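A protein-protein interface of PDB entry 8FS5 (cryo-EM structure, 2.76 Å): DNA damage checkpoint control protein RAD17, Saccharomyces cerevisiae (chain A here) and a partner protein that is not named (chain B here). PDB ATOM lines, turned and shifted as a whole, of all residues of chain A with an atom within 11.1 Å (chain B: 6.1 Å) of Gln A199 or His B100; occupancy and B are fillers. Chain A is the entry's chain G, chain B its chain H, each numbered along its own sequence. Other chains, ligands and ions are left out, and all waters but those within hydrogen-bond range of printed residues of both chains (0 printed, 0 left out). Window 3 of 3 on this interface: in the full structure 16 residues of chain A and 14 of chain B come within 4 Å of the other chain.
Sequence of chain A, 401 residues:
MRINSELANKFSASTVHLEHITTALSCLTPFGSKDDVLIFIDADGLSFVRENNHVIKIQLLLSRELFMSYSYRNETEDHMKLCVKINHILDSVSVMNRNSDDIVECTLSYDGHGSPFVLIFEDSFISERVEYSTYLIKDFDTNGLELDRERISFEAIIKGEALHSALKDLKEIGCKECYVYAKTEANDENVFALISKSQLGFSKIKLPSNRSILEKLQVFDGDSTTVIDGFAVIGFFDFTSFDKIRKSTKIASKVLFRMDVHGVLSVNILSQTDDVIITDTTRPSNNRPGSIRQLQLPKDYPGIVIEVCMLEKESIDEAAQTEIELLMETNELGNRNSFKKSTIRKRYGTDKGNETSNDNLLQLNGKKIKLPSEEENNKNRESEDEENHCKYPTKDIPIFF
The side-chain amide nitrogen of Asn B97 lies within hydrogen-bond range of a ring nitrogen (NE2) of His B100 (3.3 Å).
OG1 of Thr B103 sits at hydrogen-bond distance from O of His B100.
Of chain A, only Gln A199 (3.3 Å) and Leu A200 (3.5 Å) come within 4 Å of His B100.
No residue of chain A comes within 4 Å of Gly B98.
Arg B99 touches none of the printed residues of chain A.
No residue of chain A comes within 4 Å of Thr B102.
Of the printed residues of chain B, Glu A172 touches Thr B103 (3.4 Å).
Printed residues of chain A within 4 Å of Pro B150: Leu A200 (3.7 Å).
Printed residues of chain B within 4 Å of Leu A200: His B100 (3.5 Å), Ile B104 (3.6 Å) and Pro B150 (3.7 Å).
Leu A170 touches none of the printed residues of chain B.
Gln B151 touches none of the printed residues of chain A.
The nearest residue of chain A that does not touch His B100 is Gly A201 (6.0 Å).
Among the printed residues, pairs that only touch across the chains: Gln A199 with His B100, Leu A200 with His B100, Leu A200 with Ile B104 and Leu A200 with Pro B150.
O of Thr B103 lies close to OE2 of Glu A172 (3.4 Å).
Of the 12 printed residues of chain B, 4 touch a printed residue of chain A.
Hydrophobic or aromatic side chains of chain B that line the printed part of chain A: His B100 and Ile B104.
Among the printed residues, 5 pairs touch across the chains.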
ATOM      1  N   LYS A 168     -20.102   7.729  -7.774  1.00  0.00           N
ATOM      2  CA  LYS A 168     -20.268   7.036  -6.504  1.00  0.00           C
ATOM      3  C   LYS A 168     -18.941   6.753  -5.816  1.00  0.00           C
ATOM      4  O   LYS A 168     -18.886   6.777  -4.582  1.00  0.00           O
ATOM      5  CB  LYS A 168     -21.035   5.729  -6.714  1.00  0.00           C
ATOM      6  CG  LYS A 168     -22.538   5.861  -6.533  1.00  0.00           C
ATOM      7  CD  LYS A 168     -23.082   4.803  -5.589  1.00  0.00           C
ATOM      8  CE  LYS A 168     -24.468   5.175  -5.087  1.00  0.00           C
ATOM      9  NZ  LYS A 168     -24.420   5.827  -3.749  1.00  0.00           N
ATOM     10  N   ASP A 169     -17.878   6.485  -6.576  1.00  0.00           N
ATOM     11  CA  ASP A 169     -16.539   6.326  -6.015  1.00  0.00           C
ATOM     12  C   ASP A 169     -16.004   7.648  -5.470  1.00  0.00           C
ATOM     13  O   ASP A 169     -15.418   7.686  -4.383  1.00  0.00           O
ATOM     14  CB  ASP A 169     -15.591   5.756  -7.079  1.00  0.00           C
ATOM     15  CG  ASP A 169     -14.228   5.399  -6.518  1.00  0.00           C
ATOM     16  OD1 ASP A 169     -14.092   5.301  -5.280  1.00  0.00           O
ATOM     17  OD2 ASP A 169     -13.287   5.214  -7.317  1.00  0.00           O
ATOM     18  N   LEU A 170     -16.204   8.740  -6.211  1.00  0.00           N
ATOM     19  CA  LEU A 170     -15.801  10.052  -5.714  1.00  0.00           C
ATOM     20  C   LEU A 170     -16.542  10.410  -4.434  1.00  0.00           C
ATOM     21  O   LEU A 170     -15.953  10.983  -3.511  1.00  0.00           O
ATOM     22  CB  LEU A 170     -16.037  11.126  -6.778  1.00  0.00           C
ATOM     23  CG  LEU A 170     -15.237  11.017  -8.078  1.00  0.00           C
ATOM     24  CD1 LEU A 170     -15.567  12.174  -9.007  1.00  0.00           C
ATOM     25  CD2 LEU A 170     -13.746  10.963  -7.791  1.00  0.00           C
ATOM     26  N   LYS A 171     -17.831  10.075  -4.357  1.00  0.00           N
ATOM     27  CA  LYS A 171     -18.585  10.315  -3.131  1.00  0.00           C
ATOM     28  C   LYS A 171     -18.042   9.483  -1.974  1.00  0.00           C
ATOM     29  O   LYS A 171     -17.978   9.963  -0.836  1.00  0.00           O
ATOM     30  CB  LYS A 171     -20.066  10.019  -3.361  1.00  0.00           C
ATOM     31  CG  LYS A 171     -20.955  10.352  -2.175  1.00  0.00           C
ATOM     32  CD  LYS A 171     -20.962  11.847  -1.900  1.00  0.00           C
ATOM     33  CE  LYS A 171     -22.043  12.220  -0.901  1.00  0.00           C
ATOM     34  NZ  LYS A 171     -23.401  11.851  -1.389  1.00  0.00           N
ATOM     35  N   GLU A 172     -17.644   8.237  -2.242  1.00  0.00           N
ATOM     36  CA  GLU A 172     -17.181   7.369  -1.163  1.00  0.00           C
ATOM     37  C   GLU A 172     -15.781   7.755  -0.697  1.00  0.00           C
ATOM     38  O   GLU A 172     -15.403   7.469   0.446  1.00  0.00           O
ATOM     39  CB  GLU A 172     -17.224   5.902  -1.602  1.00  0.00           C
ATOM     40  CG  GLU A 172     -15.963   5.397  -2.288  1.00  0.00           C
ATOM     41  CD  GLU A 172     -15.985   3.900  -2.528  1.00  0.00           C
ATOM     42  OE1 GLU A 172     -16.952   3.241  -2.092  1.00  0.00           O
ATOM     43  OE2 GLU A 172     -15.035   3.383  -3.151  1.00  0.00           O
ATOM     44  N   ILE A 173     -14.996   8.404  -1.557  1.00  0.00           N
ATOM     45  CA  ILE A 173     -13.660   8.839  -1.155  1.00  0.00           C
ATOM     46  C   ILE A 173     -13.713  10.263  -0.614  1.00  0.00           C
ATOM     47  O   ILE A 173     -12.678  10.852  -0.287  1.00  0.00           O
ATOM     48  CB  ILE A 173     -12.648   8.730  -2.312  1.00  0.00           C
ATOM     49  CG1 ILE A 173     -12.936   9.786  -3.384  1.00  0.00           C
ATOM     50  CG2 ILE A 173     -12.633   7.318  -2.884  1.00  0.00           C
ATOM     51  CD1 ILE A 173     -12.152   9.592  -4.665  1.00  0.00           C
ATOM     52  N   GLY A 174     -14.917  10.818  -0.498  1.00  0.00           N
ATOM     53  CA  GLY A 174     -15.082  12.174  -0.005  1.00  0.00           C
ATOM     54  C   GLY A 174     -15.113  13.220  -1.100  1.00  0.00           C
ATOM     55  O   GLY A 174     -16.170  13.799  -1.369  1.00  0.00           O
ATOM     56  N   CYS A 175     -13.962  13.467  -1.732  1.00  0.00           N
ATOM     57  CA  CYS A 175     -13.860  14.354  -2.888  1.00  0.00           C
ATOM     58  C   CYS A 175     -14.360  15.763  -2.588  1.00  0.00           C
ATOM     59  O   CYS A 175     -15.434  16.149  -3.052  1.00  0.00           O
ATOM     60  CB  CYS A 175     -14.615  13.772  -4.087  1.00  0.00           C
ATOM     61  SG  CYS A 175     -14.415  14.695  -5.633  1.00  0.00           S
ATOM     62  N   LYS A 176     -13.635  16.513  -1.760  1.00  0.00           N
ATOM     63  CA  LYS A 176     -13.982  17.913  -1.536  1.00  0.00           C
ATOM     64  C   LYS A 176     -13.925  18.730  -2.825  1.00  0.00           C
ATOM     65  O   LYS A 176     -14.808  19.555  -3.078  1.00  0.00           O
ATOM     66  CB  LYS A 176     -13.061  18.523  -0.476  1.00  0.00           C
ATOM     67  CG  LYS A 176     -13.130  17.829   0.872  1.00  0.00           C
ATOM     68  CD  LYS A 176     -14.437  18.151   1.580  1.00  0.00           C
ATOM     69  CE  LYS A 176     -15.015  16.924   2.266  1.00  0.00           C
ATOM     70  NZ  LYS A 176     -16.480  17.059   2.501  1.00  0.00           N
ATOM     71  N   GLU A 177     -12.899  18.516  -3.645  1.00  0.00           N
ATOM     72  CA  GLU A 177     -12.758  19.182  -4.931  1.00  0.00           C
ATOM     73  C   GLU A 177     -12.511  18.149  -6.024  1.00  0.00           C
ATOM     74  O   GLU A 177     -12.043  17.037  -5.764  1.00  0.00           O
ATOM     75  CB  GLU A 177     -11.618  20.211  -4.914  1.00  0.00           C
ATOM     76  CG  GLU A 177     -11.524  21.032  -3.637  1.00  0.00           C
ATOM     77  CD  GLU A 177     -10.108  21.478  -3.333  1.00  0.00           C
ATOM     78  OE1 GLU A 177      -9.221  21.265  -4.185  1.00  0.00           O
ATOM     79  OE2 GLU A 177      -9.883  22.044  -2.243  1.00  0.00           O
ATOM     80  N   CYS A 178     -12.829  18.531  -7.261  1.00  0.00           N
ATOM     81  CA  CYS A 178     -12.733  17.623  -8.395  1.00  0.00           C
ATOM     82  C   CYS A 178     -12.064  18.320  -9.572  1.00  0.00           C
ATOM     83  O   CYS A 178     -12.114  19.545  -9.702  1.00  0.00           O
ATOM     84  CB  CYS A 178     -14.114  17.105  -8.818  1.00  0.00           C
ATOM     85  SG  CYS A 178     -14.086  15.503  -9.655  1.00  0.00           S
ATOM     86  N   ILE A 195     -10.165  13.547 -11.721  1.00  0.00           N
ATOM     87  CA  ILE A 195      -9.220  13.604 -10.609  1.00  0.00           C
ATOM     88  C   ILE A 195      -9.841  14.358  -9.435  1.00  0.00           C
ATOM     89  O   ILE A 195     -10.545  15.361  -9.599  1.00  0.00           O
ATOM     90  CB  ILE A 195      -7.895  14.244 -11.052  1.00  0.00           C
ATOM     91  CG1 ILE A 195      -7.394  13.608 -12.349  1.00  0.00           C
ATOM     92  CG2 ILE A 195      -6.836  14.080  -9.987  1.00  0.00           C
ATOM     93  CD1 ILE A 195      -7.672  14.425 -13.583  1.00  0.00           C
ATOM     94  N   SER A 196      -9.568  13.864  -8.226  1.00  0.00           N
ATOM     95  CA  SER A 196     -10.250  14.355  -7.038  1.00  0.00           C
ATOM     96  C   SER A 196      -9.256  14.750  -5.954  1.00  0.00           C
ATOM     97  O   SER A 196      -8.217  14.107  -5.782  1.00  0.00           O
ATOM     98  CB  SER A 196     -11.216  13.300  -6.486  1.00  0.00           C
ATOM     99  OG  SER A 196     -10.831  12.885  -5.186  1.00  0.00           O
ATOM    100  N   LYS A 197      -9.596  15.817  -5.230  1.00  0.00           N
ATOM    101  CA  LYS A 197      -8.952  16.207  -3.978  1.00  0.00           C
ATOM    102  C   LYS A 197      -9.845  15.770  -2.823  1.00  0.00           C
ATOM    103  O   LYS A 197     -11.033  16.107  -2.791  1.00  0.00           O
ATOM    104  CB  LYS A 197      -8.693  17.714  -3.941  1.00  0.00           C
ATOM    105  CG  LYS A 197      -7.751  18.235  -2.828  1.00  0.00           C
ATOM    106  CD  LYS A 197      -6.510  17.404  -2.464  1.00  0.00           C
ATOM    107  CE  LYS A 197      -5.648  16.964  -3.637  1.00  0.00           C
ATOM    108  NZ  LYS A 197      -4.246  16.776  -3.172  1.00  0.00           N
ATOM    109  N   SER A 198      -9.273  15.028  -1.878  1.00  0.00           N
ATOM    110  CA  SER A 198     -10.047  14.445  -0.792  1.00  0.00           C
ATOM    111  C   SER A 198      -9.127  14.210   0.402  1.00  0.00           C
ATOM    112  O   SER A 198      -7.981  14.669   0.435  1.00  0.00           O
ATOM    113  CB  SER A 198     -10.725  13.151  -1.257  1.00  0.00           C
ATOM    114  OG  SER A 198      -9.779  12.247  -1.800  1.00  0.00           O
ATOM    115  N   GLN A 199      -9.648  13.486   1.395  1.00  0.00           N
ATOM    116  CA  GLN A 199      -8.862  13.147   2.576  1.00  0.00           C
ATOM    117  C   GLN A 199      -7.740  12.177   2.228  1.00  0.00           C
ATOM    118  O   GLN A 199      -6.654  12.224   2.819  1.00  0.00           O
ATOM    119  CB  GLN A 199      -9.771  12.550   3.652  1.00  0.00           C
ATOM    120  CG  GLN A 199     -10.819  11.592   3.105  1.00  0.00           C
ATOM    121  CD  GLN A 199     -11.801  11.127   4.163  1.00  0.00           C
ATOM    122  OE1 GLN A 199     -11.784  11.606   5.296  1.00  0.00           O
ATOM    123  NE2 GLN A 199     -12.663  10.186   3.796  1.00  0.00           N
ATOM    124  N   LEU A 200      -7.994  11.280   1.275  1.00  0.00           N
ATOM    125  CA  LEU A 200      -7.038  10.257   0.864  1.00  0.00           C
ATOM    126  C   LEU A 200      -5.739  10.850   0.335  1.00  0.00           C
ATOM    127  O   LEU A 200      -4.648  10.402   0.700  1.00  0.00           O
ATOM    128  CB  LEU A 200      -7.661   9.364  -0.210  1.00  0.00           C
ATOM    129  CG  LEU A 200      -8.274   8.046   0.252  1.00  0.00           C
ATOM    130  CD1 LEU A 200      -9.216   7.497  -0.802  1.00  0.00           C
ATOM    131  CD2 LEU A 200      -7.156   7.068   0.526  1.00  0.00           C
ATOM    132  N   GLY A 201      -5.851  11.858  -0.520  1.00  0.00           N
ATOM    133  CA  GLY A 201      -4.700  12.389  -1.216  1.00  0.00           C
ATOM    134  C   GLY A 201      -5.098  12.931  -2.570  1.00  0.00           C
ATOM    135  O   GLY A 201      -5.990  13.779  -2.664  1.00  0.00           O
ATOM    136  N   PHE A 202      -4.450  12.455  -3.629  1.00  0.00           N
ATOM    137  CA  PHE A 202      -4.764  12.901  -4.980  1.00  0.00           C
ATOM    138  C   PHE A 202      -5.166  11.678  -5.799  1.00  0.00           C
ATOM    139  O   PHE A 202      -4.306  10.964  -6.324  1.00  0.00           O
ATOM    140  CB  PHE A 202      -3.566  13.614  -5.598  1.00  0.00           C
ATOM    141  CG  PHE A 202      -3.916  14.916  -6.252  1.00  0.00           C
ATOM    142  CD1 PHE A 202      -4.990  15.012  -7.114  1.00  0.00           C
ATOM    143  CD2 PHE A 202      -3.165  16.050  -5.999  1.00  0.00           C
ATOM    144  CE1 PHE A 202      -5.312  16.218  -7.699  1.00  0.00           C
ATOM    145  CE2 PHE A 202      -3.481  17.258  -6.587  1.00  0.00           C
ATOM    146  CZ  PHE A 202      -4.553  17.341  -7.442  1.00  0.00           C
ATOM    147  N   SER A 203      -6.469  11.439  -5.913  1.00  0.00           N
ATOM    148  CA  SER A 203      -6.989  10.232  -6.538  1.00  0.00           C
ATOM    149  C   SER A 203      -7.503  10.526  -7.941  1.00  0.00           C
ATOM    150  O   SER A 203      -8.016  11.611  -8.228  1.00  0.00           O
ATOM    151  CB  SER A 203      -8.109   9.616  -5.691  1.00  0.00           C
ATOM    152  OG  SER A 203      -9.004   8.870  -6.496  1.00  0.00           O
ATOM    153  N   PHE A 239     -17.139  19.583  -5.955  1.00  0.00           N
ATOM    154  CA  PHE A 239     -17.900  18.341  -6.025  1.00  0.00           C
ATOM    155  C   PHE A 239     -19.286  18.472  -5.412  1.00  0.00           C
ATOM    156  O   PHE A 239     -20.130  17.600  -5.634  1.00  0.00           O
ATOM    157  CB  PHE A 239     -17.126  17.214  -5.347  1.00  0.00           C
ATOM    158  CG  PHE A 239     -17.724  15.851  -5.555  1.00  0.00           C
ATOM    159  CD1 PHE A 239     -17.768  15.281  -6.817  1.00  0.00           C
ATOM    160  CD2 PHE A 239     -18.245  15.139  -4.487  1.00  0.00           C
ATOM    161  CE1 PHE A 239     -18.319  14.028  -7.009  1.00  0.00           C
ATOM    162  CE2 PHE A 239     -18.796  13.886  -4.672  1.00  0.00           C
ATOM    163  CZ  PHE A 239     -18.833  13.329  -5.935  1.00  0.00           C
ATOM    164  N   VAL B  96      -0.272   3.555   7.537  1.00  0.00           N
ATOM    165  CA  VAL B  96      -1.284   4.053   6.611  1.00  0.00           C
ATOM    166  C   VAL B  96      -2.615   4.125   7.348  1.00  0.00           C
ATOM    167  O   VAL B  96      -2.910   3.287   8.205  1.00  0.00           O
ATOM    168  CB  VAL B  96      -1.367   3.171   5.342  1.00  0.00           C
ATOM    169  CG1 VAL B  96      -1.765   1.743   5.693  1.00  0.00           C
ATOM    170  CG2 VAL B  96      -2.321   3.773   4.316  1.00  0.00           C
ATOM    171  N   ASN B  97      -3.403   5.153   7.035  1.00  0.00           N
ATOM    172  CA  ASN B  97      -4.697   5.337   7.681  1.00  0.00           C
ATOM    173  C   ASN B  97      -5.633   4.185   7.337  1.00  0.00           C
ATOM    174  O   ASN B  97      -5.815   3.843   6.165  1.00  0.00           O
ATOM    175  CB  ASN B  97      -5.313   6.669   7.250  1.00  0.00           C
ATOM    176  CG  ASN B  97      -6.465   7.098   8.142  1.00  0.00           C
ATOM    177  OD1 ASN B  97      -6.895   6.358   9.026  1.00  0.00           O
ATOM    178  ND2 ASN B  97      -6.974   8.303   7.909  1.00  0.00           N
ATOM    179  N   GLY B  98      -6.222   3.584   8.368  1.00  0.00           N
ATOM    180  CA  GLY B  98      -7.126   2.467   8.181  1.00  0.00           C
ATOM    181  C   GLY B  98      -8.426   2.822   7.491  1.00  0.00           C
ATOM    182  O   GLY B  98      -8.877   2.102   6.594  1.00  0.00           O
ATOM    183  N   ARG B  99      -9.036   3.934   7.907  1.00  0.00           N
ATOM    184  CA  ARG B  99     -10.287   4.371   7.301  1.00  0.00           C
ATOM    185  C   ARG B  99     -10.107   4.782   5.847  1.00  0.00           C
ATOM    186  O   ARG B  99     -11.078   4.761   5.084  1.00  0.00           O
ATOM    187  CB  ARG B  99     -10.881   5.531   8.100  1.00  0.00           C
ATOM    188  CG  ARG B  99     -11.807   5.098   9.226  1.00  0.00           C
ATOM    189  CD  ARG B  99     -12.334   6.261  10.077  1.00  0.00           C
ATOM    190  NE  ARG B  99     -11.321   7.247  10.441  1.00  0.00           N
ATOM    191  CZ  ARG B  99     -11.083   8.370   9.774  1.00  0.00           C
ATOM    192  NH1 ARG B  99     -11.779   8.694   8.697  1.00  0.00           N
ATOM    193  NH2 ARG B  99     -10.124   9.187  10.200  1.00  0.00           N
ATOM    194  N   HIS B 100      -8.893   5.158   5.451  1.00  0.00           N
ATOM    195  CA  HIS B 100      -8.603   5.499   4.066  1.00  0.00           C
ATOM    196  C   HIS B 100      -8.344   4.265   3.211  1.00  0.00           C
ATOM    197  O   HIS B 100      -8.794   4.202   2.062  1.00  0.00           O
ATOM    198  CB  HIS B 100      -7.401   6.443   4.004  1.00  0.00           C
ATOM    199  CG  HIS B 100      -7.688   7.819   4.521  1.00  0.00           C
ATOM    200  ND1 HIS B 100      -6.743   8.822   4.530  1.00  0.00           N
ATOM    201  CD2 HIS B 100      -8.814   8.358   5.044  1.00  0.00           C
ATOM    202  CE1 HIS B 100      -7.275   9.920   5.038  1.00  0.00           C
ATOM    203  NE2 HIS B 100      -8.531   9.664   5.358  1.00  0.00           N
ATOM    204  N   LEU B 101      -7.624   3.279   3.750  1.00  0.00           N
ATOM    205  CA  LEU B 101      -7.354   2.052   3.012  1.00  0.00           C
ATOM    206  C   LEU B 101      -8.569   1.136   2.935  1.00  0.00           C
ATOM    207  O   LEU B 101      -8.663   0.333   2.000  1.00  0.00           O
ATOM    208  CB  LEU B 101      -6.180   1.305   3.649  1.00  0.00           C
ATOM    209  CG  LEU B 101      -5.544   0.173   2.838  1.00  0.00           C
ATOM    210  CD1 LEU B 101      -4.998   0.695   1.518  1.00  0.00           C
ATOM    211  CD2 LEU B 101      -4.448  -0.513   3.638  1.00  0.00           C
ATOM    212  N   THR B 102      -9.502   1.241   3.880  1.00  0.00           N
ATOM    213  CA  THR B 102     -10.693   0.401   3.874  1.00  0.00           C
ATOM    214  C   THR B 102     -11.711   0.824   2.820  1.00  0.00           C
ATOM    215  O   THR B 102     -12.634   0.054   2.532  1.00  0.00           O
ATOM    216  CB  THR B 102     -11.350   0.402   5.258  1.00  0.00           C
ATOM    217  OG1 THR B 102     -12.206  -0.741   5.382  1.00  0.00           O
ATOM    218  CG2 THR B 102     -12.170   1.665   5.463  1.00  0.00           C
ATOM    219  N   THR B 103     -11.570   2.013   2.242  1.00  0.00           N
ATOM    220  CA  THR B 103     -12.431   2.458   1.154  1.00  0.00           C
ATOM    221  C   THR B 103     -11.829   2.200  -0.216  1.00  0.00           C
ATOM    222  O   THR B 103     -12.571   1.992  -1.180  1.00  0.00           O
ATOM    223  CB  THR B 103     -12.750   3.954   1.294  1.00  0.00           C
ATOM    224  OG1 THR B 103     -11.580   4.727   1.003  1.00  0.00           O
ATOM    225  CG2 THR B 103     -13.230   4.269   2.702  1.00  0.00           C
ATOM    226  N   ILE B 104     -10.499   2.214  -0.331  1.00  0.00           N
ATOM    227  CA  ILE B 104      -9.853   1.812  -1.573  1.00  0.00           C
ATOM    228  C   ILE B 104     -10.088   0.340  -1.860  1.00  0.00           C
ATOM    229  O   ILE B 104     -10.428  -0.027  -2.990  1.00  0.00           O
ATOM    230  CB  ILE B 104      -8.342   2.113  -1.524  1.00  0.00           C
ATOM    231  CG1 ILE B 104      -8.086   3.587  -1.221  1.00  0.00           C
ATOM    232  CG2 ILE B 104      -7.688   1.737  -2.837  1.00  0.00           C
ATOM    233  CD1 ILE B 104      -6.614   3.924  -1.131  1.00  0.00           C
ATOM    234  N   SER B 105      -9.926  -0.519  -0.853  1.00  0.00           N
ATOM    235  CA  SER B 105     -10.123  -1.952  -1.016  1.00  0.00           C
ATOM    236  C   SER B 105     -11.586  -2.363  -0.979  1.00  0.00           C
ATOM    237  O   SER B 105     -11.886  -3.543  -1.193  1.00  0.00           O
ATOM    238  CB  SER B 105      -9.359  -2.719   0.070  1.00  0.00           C
ATOM    239  OG  SER B 105      -9.894  -2.454   1.355  1.00  0.00           O
ATOM    240  N   PRO B 150      -2.550   7.164  -1.308  1.00  0.00           N
ATOM    241  CA  PRO B 150      -2.596   7.370   0.146  1.00  0.00           C
ATOM    242  C   PRO B 150      -1.211   7.644   0.714  1.00  0.00           C
ATOM    243  O   PRO B 150      -0.237   6.966   0.381  1.00  0.00           O
ATOM    244  CB  PRO B 150      -3.174   6.051   0.672  1.00  0.00           C
ATOM    245  CG  PRO B 150      -2.823   5.052  -0.371  1.00  0.00           C
ATOM    246  CD  PRO B 150      -2.923   5.786  -1.673  1.00  0.00           C
ATOM    247  N   GLN B 151      -1.135   8.650   1.580  1.00  0.00           N
ATOM    248  CA  GLN B 151       0.116   8.992   2.243  1.00  0.00           C
ATOM    249  C   GLN B 151       0.465   7.964   3.315  1.00  0.00           C
ATOM    250  O   GLN B 151      -0.410   7.466   4.029  1.00  0.00           O
ATOM    251  CB  GLN B 151       0.009  10.395   2.847  1.00  0.00           C
ATOM    252  CG  GLN B 151      -1.153  10.564   3.821  1.00  0.00           C
ATOM    253  CD  GLN B 151      -0.967  11.730   4.769  1.00  0.00           C
ATOM    254  OE1 GLN B 151      -0.721  11.542   5.960  1.00  0.00           O
ATOM    255  NE2 GLN B 151      -1.062  12.943   4.241  1.00  0.00           N
